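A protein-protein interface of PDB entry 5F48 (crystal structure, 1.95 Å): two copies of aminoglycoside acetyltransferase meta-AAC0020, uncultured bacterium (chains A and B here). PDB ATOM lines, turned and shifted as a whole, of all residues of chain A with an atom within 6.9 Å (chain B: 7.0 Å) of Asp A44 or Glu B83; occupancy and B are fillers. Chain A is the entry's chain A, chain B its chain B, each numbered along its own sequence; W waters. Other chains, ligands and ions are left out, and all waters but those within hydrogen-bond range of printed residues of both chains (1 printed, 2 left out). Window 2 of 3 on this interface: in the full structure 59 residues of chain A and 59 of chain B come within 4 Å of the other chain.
NE2 of His A47 lies within hydrogen-bond range of O of Gln B79 (2.7 Å). A ring nitrogen (NE2) of His A47 is in hydrogen-bond range of the backbone carbonyl oxygen of Ser B82 (3.2 Å). The side-chain carboxylate of Asp A44 sits close to the side-chain carboxylate of Glu B83, 2.8 Å away.
Asp A44 touches one residue of chain B. Of chain A, only Asp A44 and His A47 come within 4 Å of Glu B83. Printed residues of chain A within 4 Å of Tyr B81: Pro A43. Printed residues of chain A within 4 Å of Glu B78: His A47. Of the printed residues of chain B, His A47 touches Glu B78 (3.3 Å), Gln B79 (2.7 Å), Ser B82 (3.2 Å) and Glu B83 (3.7 Å). Gln A49 touches none of the printed residues of chain B. Glu A46 touches none of the printed residues of chain B. The nearest printed residue of chain B that does not touch Asp A44 is Ser B82 (7.2 Å). The nearest residue of chain A that does not touch Glu B83 is Pro A43 (4.3 Å). The nearest printed residue of chain A that does not touch Glu B78 is Lys A50 (4.6 Å).
OD1 of Asp A44 sits at hydrogen-bond distance from N of His A47, at 2.9 Å. NE2 of Gln B79 lies within hydrogen-bond range of O of Lys B84 (2.5 Å). The side-chain amide nitrogen of Gln B79 is in hydrogen-bond range of the side-chain carboxylate of Glu B121. N of Lys B84 sits at hydrogen-bond distance from OG of Ser B82.
Among the printed residues, merely in contact across the chains: Pro A43 with Tyr B80, His A47 with Glu B78, Pro A43 with Ser B82, His A47 with Glu B83, Pro A43 with Tyr B81 and Leu A48 with Tyr B80.
Water W1 lies within hydrogen-bond range of the backbone carbonyl oxygen (O) of Tyr B81 and the backbone carbonyl oxygen (O) of Ser A41.
Hydrophobic or aromatic side chains of chain A that line the printed part of chain B: Pro A43, His A47 and Leu A48. Printed residues of chain B that touch a printed residue of chain A: Glu B78, Gln B79, Tyr B80, Tyr B81, Ser B82 and Glu B83. Hydrophobic or aromatic side chains of chain B that line the printed part of chain A: Tyr B80. Among the printed residues, no Asp or Glu carboxylate lies within 4 Å of a Lys or Arg side-chain nitrogen of the other chain.
No position is printed for both chains. Of the 9 pairs that touch across the chains among the printed residues, none has its exchanged pair printed and touching as well.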
ATOM      1  N   LEU A  21      12.929  -0.111  26.723  1.00  0.00           N
ATOM      2  CA  LEU A  21      13.947  -1.128  27.054  1.00  0.00           C
ATOM      3  C   LEU A  21      14.837  -0.772  28.268  1.00  0.00           C
ATOM      4  O   LEU A  21      15.022  -1.610  29.137  1.00  0.00           O
ATOM      5  CB  LEU A  21      14.836  -1.432  25.836  1.00  0.00           C
ATOM      6  CG  LEU A  21      16.024  -2.389  26.051  1.00  0.00           C
ATOM      7  CD1 LEU A  21      15.581  -3.766  26.507  1.00  0.00           C
ATOM      8  CD2 LEU A  21      16.876  -2.533  24.805  1.00  0.00           C
ATOM      9  N   SER A  41      23.223 -14.096  33.983  1.00  0.00           N
ATOM     10  CA  SER A  41      23.692 -13.422  32.772  1.00  0.00           C
ATOM     11  C   SER A  41      22.468 -12.935  32.016  1.00  0.00           C
ATOM     12  O   SER A  41      21.661 -13.744  31.557  1.00  0.00           O
ATOM     13  CB  SER A  41      24.532 -14.358  31.895  1.00  0.00           C
ATOM     14  OG  SER A  41      25.637 -14.898  32.603  1.00  0.00           O
ATOM     15  N   ILE A  42      22.302 -11.622  31.920  1.00  0.00           N
ATOM     16  CA  ILE A  42      21.088 -11.062  31.339  1.00  0.00           C
ATOM     17  C   ILE A  42      21.057 -11.381  29.850  1.00  0.00           C
ATOM     18  O   ILE A  42      22.080 -11.337  29.194  1.00  0.00           O
ATOM     19  CB  ILE A  42      21.006  -9.539  31.578  1.00  0.00           C
ATOM     20  CG1 ILE A  42      19.593  -9.022  31.295  1.00  0.00           C
ATOM     21  CG2 ILE A  42      22.056  -8.797  30.737  1.00  0.00           C
ATOM     22  CD1 ILE A  42      19.344  -7.604  31.742  1.00  0.00           C
ATOM     23  N   PRO A  43      19.887 -11.758  29.320  1.00  0.00           N
ATOM     24  CA  PRO A  43      19.742 -11.993  27.873  1.00  0.00           C
ATOM     25  C   PRO A  43      20.136 -10.776  27.039  1.00  0.00           C
ATOM     26  O   PRO A  43      20.104  -9.656  27.565  1.00  0.00           O
ATOM     27  CB  PRO A  43      18.249 -12.288  27.717  1.00  0.00           C
ATOM     28  CG  PRO A  43      17.864 -12.917  29.000  1.00  0.00           C
ATOM     29  CD  PRO A  43      18.724 -12.256  30.076  1.00  0.00           C
ATOM     30  N   ASP A  44      20.482 -10.976  25.768  1.00  0.00           N
ATOM     31  CA  ASP A  44      20.925  -9.848  24.956  1.00  0.00           C
ATOM     32  C   ASP A  44      19.753  -8.908  24.711  1.00  0.00           C
ATOM     33  O   ASP A  44      18.591  -9.298  24.820  1.00  0.00           O
ATOM     34  CB  ASP A  44      21.587 -10.304  23.637  1.00  0.00           C
ATOM     35  CG  ASP A  44      20.678 -11.138  22.740  1.00  0.00           C
ATOM     36  OD1 ASP A  44      19.465 -10.857  22.653  1.00  0.00           O
ATOM     37  OD2 ASP A  44      21.200 -12.070  22.079  1.00  0.00           O
ATOM     38  N   SER A  45      20.062  -7.654  24.412  1.00  0.00           N
ATOM     39  CA  SER A  45      19.035  -6.630  24.369  1.00  0.00           C
ATOM     40  C   SER A  45      18.077  -6.831  23.213  1.00  0.00           C
ATOM     41  O   SER A  45      16.929  -6.398  23.282  1.00  0.00           O
ATOM     42  CB  SER A  45      19.676  -5.240  24.300  1.00  0.00           C
ATOM     43  OG  SER A  45      20.331  -4.952  25.526  1.00  0.00           O
ATOM     44  N   GLU A  46      18.532  -7.486  22.151  1.00  0.00           N
ATOM     45  CA  GLU A  46      17.638  -7.774  21.033  1.00  0.00           C
ATOM     46  C   GLU A  46      16.509  -8.713  21.499  1.00  0.00           C
ATOM     47  O   GLU A  46      15.350  -8.507  21.159  1.00  0.00           O
ATOM     48  CB  GLU A  46      18.427  -8.343  19.850  1.00  0.00           C
ATOM     49  CG  GLU A  46      19.333  -7.278  19.197  1.00  0.00           C
ATOM     50  CD  GLU A  46      20.263  -7.822  18.113  1.00  0.00           C
ATOM     51  OE1 GLU A  46      20.373  -9.060  17.970  1.00  0.00           O
ATOM     52  OE2 GLU A  46      20.903  -7.005  17.412  1.00  0.00           O
ATOM     53  N   HIS A  47      16.838  -9.701  22.324  1.00  0.00           N
ATOM     54  CA  HIS A  47      15.811 -10.607  22.847  1.00  0.00           C
ATOM     55  C   HIS A  47      14.798  -9.871  23.720  1.00  0.00           C
ATOM     56  O   HIS A  47      13.577 -10.025  23.557  1.00  0.00           O
ATOM     57  CB  HIS A  47      16.440 -11.749  23.645  1.00  0.00           C
ATOM     58  CG  HIS A  47      15.430 -12.666  24.264  1.00  0.00           C
ATOM     59  ND1 HIS A  47      14.770 -13.637  23.544  1.00  0.00           N
ATOM     60  CD2 HIS A  47      14.959 -12.752  25.531  1.00  0.00           C
ATOM     61  CE1 HIS A  47      13.937 -14.282  24.342  1.00  0.00           C
ATOM     62  NE2 HIS A  47      14.033 -13.766  25.552  1.00  0.00           N
ATOM     63  N   LEU A  48      15.309  -9.065  24.647  1.00  0.00           N
ATOM     64  CA  LEU A  48      14.469  -8.323  25.574  1.00  0.00           C
ATOM     65  C   LEU A  48      13.578  -7.340  24.814  1.00  0.00           C
ATOM     66  O   LEU A  48      12.410  -7.189  25.121  1.00  0.00           O
ATOM     67  CB  LEU A  48      15.343  -7.593  26.615  1.00  0.00           C
ATOM     68  CG  LEU A  48      16.200  -8.496  27.529  1.00  0.00           C
ATOM     69  CD1 LEU A  48      17.009  -7.664  28.558  1.00  0.00           C
ATOM     70  CD2 LEU A  48      15.384  -9.553  28.258  1.00  0.00           C
ATOM     71  N   GLN A  49      14.126  -6.695  23.791  1.00  0.00           N
ATOM     72  CA  GLN A  49      13.344  -5.751  23.000  1.00  0.00           C
ATOM     73  C   GLN A  49      12.162  -6.453  22.331  1.00  0.00           C
ATOM     74  O   GLN A  49      11.034  -5.953  22.352  1.00  0.00           O
ATOM     75  CB  GLN A  49      14.218  -5.077  21.937  1.00  0.00           C
ATOM     76  CG  GLN A  49      13.447  -4.060  21.051  1.00  0.00           C
ATOM     77  CD  GLN A  49      12.941  -2.868  21.853  1.00  0.00           C
ATOM     78  OE1 GLN A  49      13.724  -2.064  22.335  1.00  0.00           O
ATOM     79  NE2 GLN A  49      11.632  -2.754  21.995  1.00  0.00           N
ATOM     80  N   LYS A  50      12.444  -7.607  21.724  1.00  0.00           N
ATOM     81  CA  LYS A  50      11.431  -8.395  21.024  1.00  0.00           C
ATOM     82  C   LYS A  50      10.300  -8.749  21.992  1.00  0.00           C
ATOM     83  O   LYS A  50       9.124  -8.653  21.641  1.00  0.00           O
ATOM     84  CB  LYS A  50      12.061  -9.645  20.424  1.00  0.00           C
ATOM     85  CG  LYS A  50      11.133 -10.500  19.579  1.00  0.00           C
ATOM     86  CD  LYS A  50      11.940 -11.372  18.613  1.00  0.00           C
ATOM     87  CE  LYS A  50      13.077 -12.118  19.331  1.00  0.00           C
ATOM     88  NZ  LYS A  50      12.614 -13.241  20.220  1.00  0.00           N
ATOM     89  N   GLU B  78       7.579 -16.378  26.656  1.00  0.00           N
ATOM     90  CA  GLU B  78       8.939 -15.933  26.413  1.00  0.00           C
ATOM     91  C   GLU B  78       9.500 -15.320  27.693  1.00  0.00           C
ATOM     92  O   GLU B  78       8.798 -14.593  28.406  1.00  0.00           O
ATOM     93  CB  GLU B  78       8.986 -14.934  25.255  1.00  0.00           C
ATOM     94  CG  GLU B  78       8.710 -15.554  23.888  1.00  0.00           C
ATOM     95  CD  GLU B  78       9.977 -15.993  23.152  1.00  0.00           C
ATOM     96  OE1 GLU B  78      11.095 -15.822  23.690  1.00  0.00           O
ATOM     97  OE2 GLU B  78       9.849 -16.495  22.014  1.00  0.00           O
ATOM     98  N   GLN B  79      10.761 -15.631  27.980  1.00  0.00           N
ATOM     99  CA  GLN B  79      11.399 -15.218  29.220  1.00  0.00           C
ATOM    100  C   GLN B  79      12.331 -14.017  29.046  1.00  0.00           C
ATOM    101  O   GLN B  79      12.868 -13.783  27.955  1.00  0.00           O
ATOM    102  CB  GLN B  79      12.203 -16.360  29.813  1.00  0.00           C
ATOM    103  CG  GLN B  79      11.427 -17.618  30.115  1.00  0.00           C
ATOM    104  CD  GLN B  79      12.266 -18.558  30.949  1.00  0.00           C
ATOM    105  OE1 GLN B  79      12.379 -18.379  32.159  1.00  0.00           O
ATOM    106  NE2 GLN B  79      12.894 -19.539  30.303  1.00  0.00           N
ATOM    107  N   TYR B  80      12.507 -13.279  30.145  1.00  0.00           N
ATOM    108  CA  TYR B  80      13.506 -12.217  30.236  1.00  0.00           C
ATOM    109  C   TYR B  80      14.698 -12.677  31.067  1.00  0.00           C
ATOM    110  O   TYR B  80      15.719 -11.990  31.119  1.00  0.00           O
ATOM    111  CB  TYR B  80      12.899 -10.942  30.829  1.00  0.00           C
ATOM    112  CG  TYR B  80      11.924 -11.163  31.972  1.00  0.00           C
ATOM    113  CD1 TYR B  80      12.363 -11.237  33.289  1.00  0.00           C
ATOM    114  CD2 TYR B  80      10.558 -11.288  31.730  1.00  0.00           C
ATOM    115  CE1 TYR B  80      11.462 -11.431  34.335  1.00  0.00           C
ATOM    116  CE2 TYR B  80       9.662 -11.486  32.755  1.00  0.00           C
ATOM    117  CZ  TYR B  80      10.113 -11.552  34.051  1.00  0.00           C
ATOM    118  OH  TYR B  80       9.208 -11.722  35.064  1.00  0.00           O
ATOM    119  N   TYR B  81      14.580 -13.838  31.718  1.00  0.00           N
ATOM    120  CA  TYR B  81      15.730 -14.435  32.424  1.00  0.00           C
ATOM    121  C   TYR B  81      16.568 -15.320  31.489  1.00  0.00           C
ATOM    122  O   TYR B  81      17.669 -15.759  31.838  1.00  0.00           O
ATOM    123  CB  TYR B  81      15.275 -15.280  33.629  1.00  0.00           C
ATOM    124  CG  TYR B  81      14.605 -14.501  34.752  1.00  0.00           C
ATOM    125  CD1 TYR B  81      15.144 -13.305  35.221  1.00  0.00           C
ATOM    126  CD2 TYR B  81      13.413 -14.948  35.315  1.00  0.00           C
ATOM    127  CE1 TYR B  81      14.535 -12.594  36.236  1.00  0.00           C
ATOM    128  CE2 TYR B  81      12.795 -14.239  36.325  1.00  0.00           C
ATOM    129  CZ  TYR B  81      13.363 -13.064  36.787  1.00  0.00           C
ATOM    130  OH  TYR B  81      12.750 -12.350  37.789  1.00  0.00           O
ATOM    131  N   SER B  82      16.034 -15.587  30.305  1.00  0.00           N
ATOM    132  CA  SER B  82      16.643 -16.526  29.382  1.00  0.00           C
ATOM    133  C   SER B  82      16.126 -16.288  27.973  1.00  0.00           C
ATOM    134  O   SER B  82      15.030 -15.771  27.789  1.00  0.00           O
ATOM    135  CB  SER B  82      16.343 -17.976  29.813  1.00  0.00           C
ATOM    136  OG  SER B  82      16.852 -18.901  28.864  1.00  0.00           O
ATOM    137  N   GLU B  83      16.917 -16.666  26.979  1.00  0.00           N
ATOM    138  CA  GLU B  83      16.449 -16.673  25.601  1.00  0.00           C
ATOM    139  C   GLU B  83      15.600 -17.898  25.324  1.00  0.00           C
ATOM    140  O   GLU B  83      14.875 -17.945  24.337  1.00  0.00           O
ATOM    141  CB  GLU B  83      17.626 -16.627  24.631  1.00  0.00           C
ATOM    142  CG  GLU B  83      18.535 -15.440  24.865  1.00  0.00           C
ATOM    143  CD  GLU B  83      19.150 -14.924  23.582  1.00  0.00           C
ATOM    144  OE1 GLU B  83      18.820 -15.471  22.501  1.00  0.00           O
ATOM    145  OE2 GLU B  83      19.957 -13.975  23.663  1.00  0.00           O
ATOM    146  N   LYS B  84      15.685 -18.889  26.204  1.00  0.00           N
ATOM    147  CA  LYS B  84      14.880 -20.099  26.073  1.00  0.00           C
ATOM    148  C   LYS B  84      13.510 -19.915  26.705  1.00  0.00           C
ATOM    149  O   LYS B  84      13.403 -19.660  27.902  1.00  0.00           O
ATOM    150  CB  LYS B  84      15.586 -21.294  26.720  1.00  0.00           C
ATOM    151  CG  LYS B  84      16.941 -21.614  26.123  1.00  0.00           C
ATOM    152  CD  LYS B  84      17.416 -22.964  26.622  1.00  0.00           C
ATOM    153  CE  LYS B  84      18.607 -23.461  25.843  1.00  0.00           C
ATOM    154  NZ  LYS B  84      18.798 -24.923  26.048  1.00  0.00           N
ATOM    155  N   PRO B  85      12.450 -20.062  25.902  1.00  0.00           N
ATOM    156  CA  PRO B  85      11.116 -19.851  26.460  1.00  0.00           C
ATOM    157  C   PRO B  85      10.614 -20.998  27.353  1.00  0.00           C
ATOM    158  O   PRO B  85      11.223 -22.073  27.409  1.00  0.00           O
ATOM    159  CB  PRO B  85      10.243 -19.677  25.217  1.00  0.00           C
ATOM    160  CG  PRO B  85      11.027 -20.245  24.081  1.00  0.00           C
ATOM    161  CD  PRO B  85      12.456 -20.173  24.434  1.00  0.00           C
ATOM    162  N   GLY B 119      13.580 -26.111  21.650  1.00  0.00           N
ATOM    163  CA  GLY B 119      14.638 -25.536  22.459  1.00  0.00           C
ATOM    164  C   GLY B 119      14.158 -24.753  23.675  1.00  0.00           C
ATOM    165  O   GLY B 119      14.862 -23.880  24.173  1.00  0.00           O
ATOM    166  N   GLU B 121      13.225 -24.027  27.621  1.00  0.00           N
ATOM    167  CA  GLU B 121      13.889 -24.372  28.868  1.00  0.00           C
ATOM    168  C   GLU B 121      13.110 -25.420  29.673  1.00  0.00           C
ATOM    169  O   GLU B 121      13.700 -26.316  30.272  1.00  0.00           O
ATOM    170  CB  GLU B 121      14.095 -23.122  29.720  1.00  0.00           C
ATOM    171  CG  GLU B 121      14.758 -23.387  31.042  1.00  0.00           C
ATOM    172  CD  GLU B 121      14.808 -22.153  31.916  1.00  0.00           C
ATOM    173  OE1 GLU B 121      14.610 -21.036  31.390  1.00  0.00           O
ATOM    174  OE2 GLU B 121      15.044 -22.303  33.130  1.00  0.00           O
HETATM  175  O   HOH W   1      20.197 -15.920  31.273  1.00  0.00           O
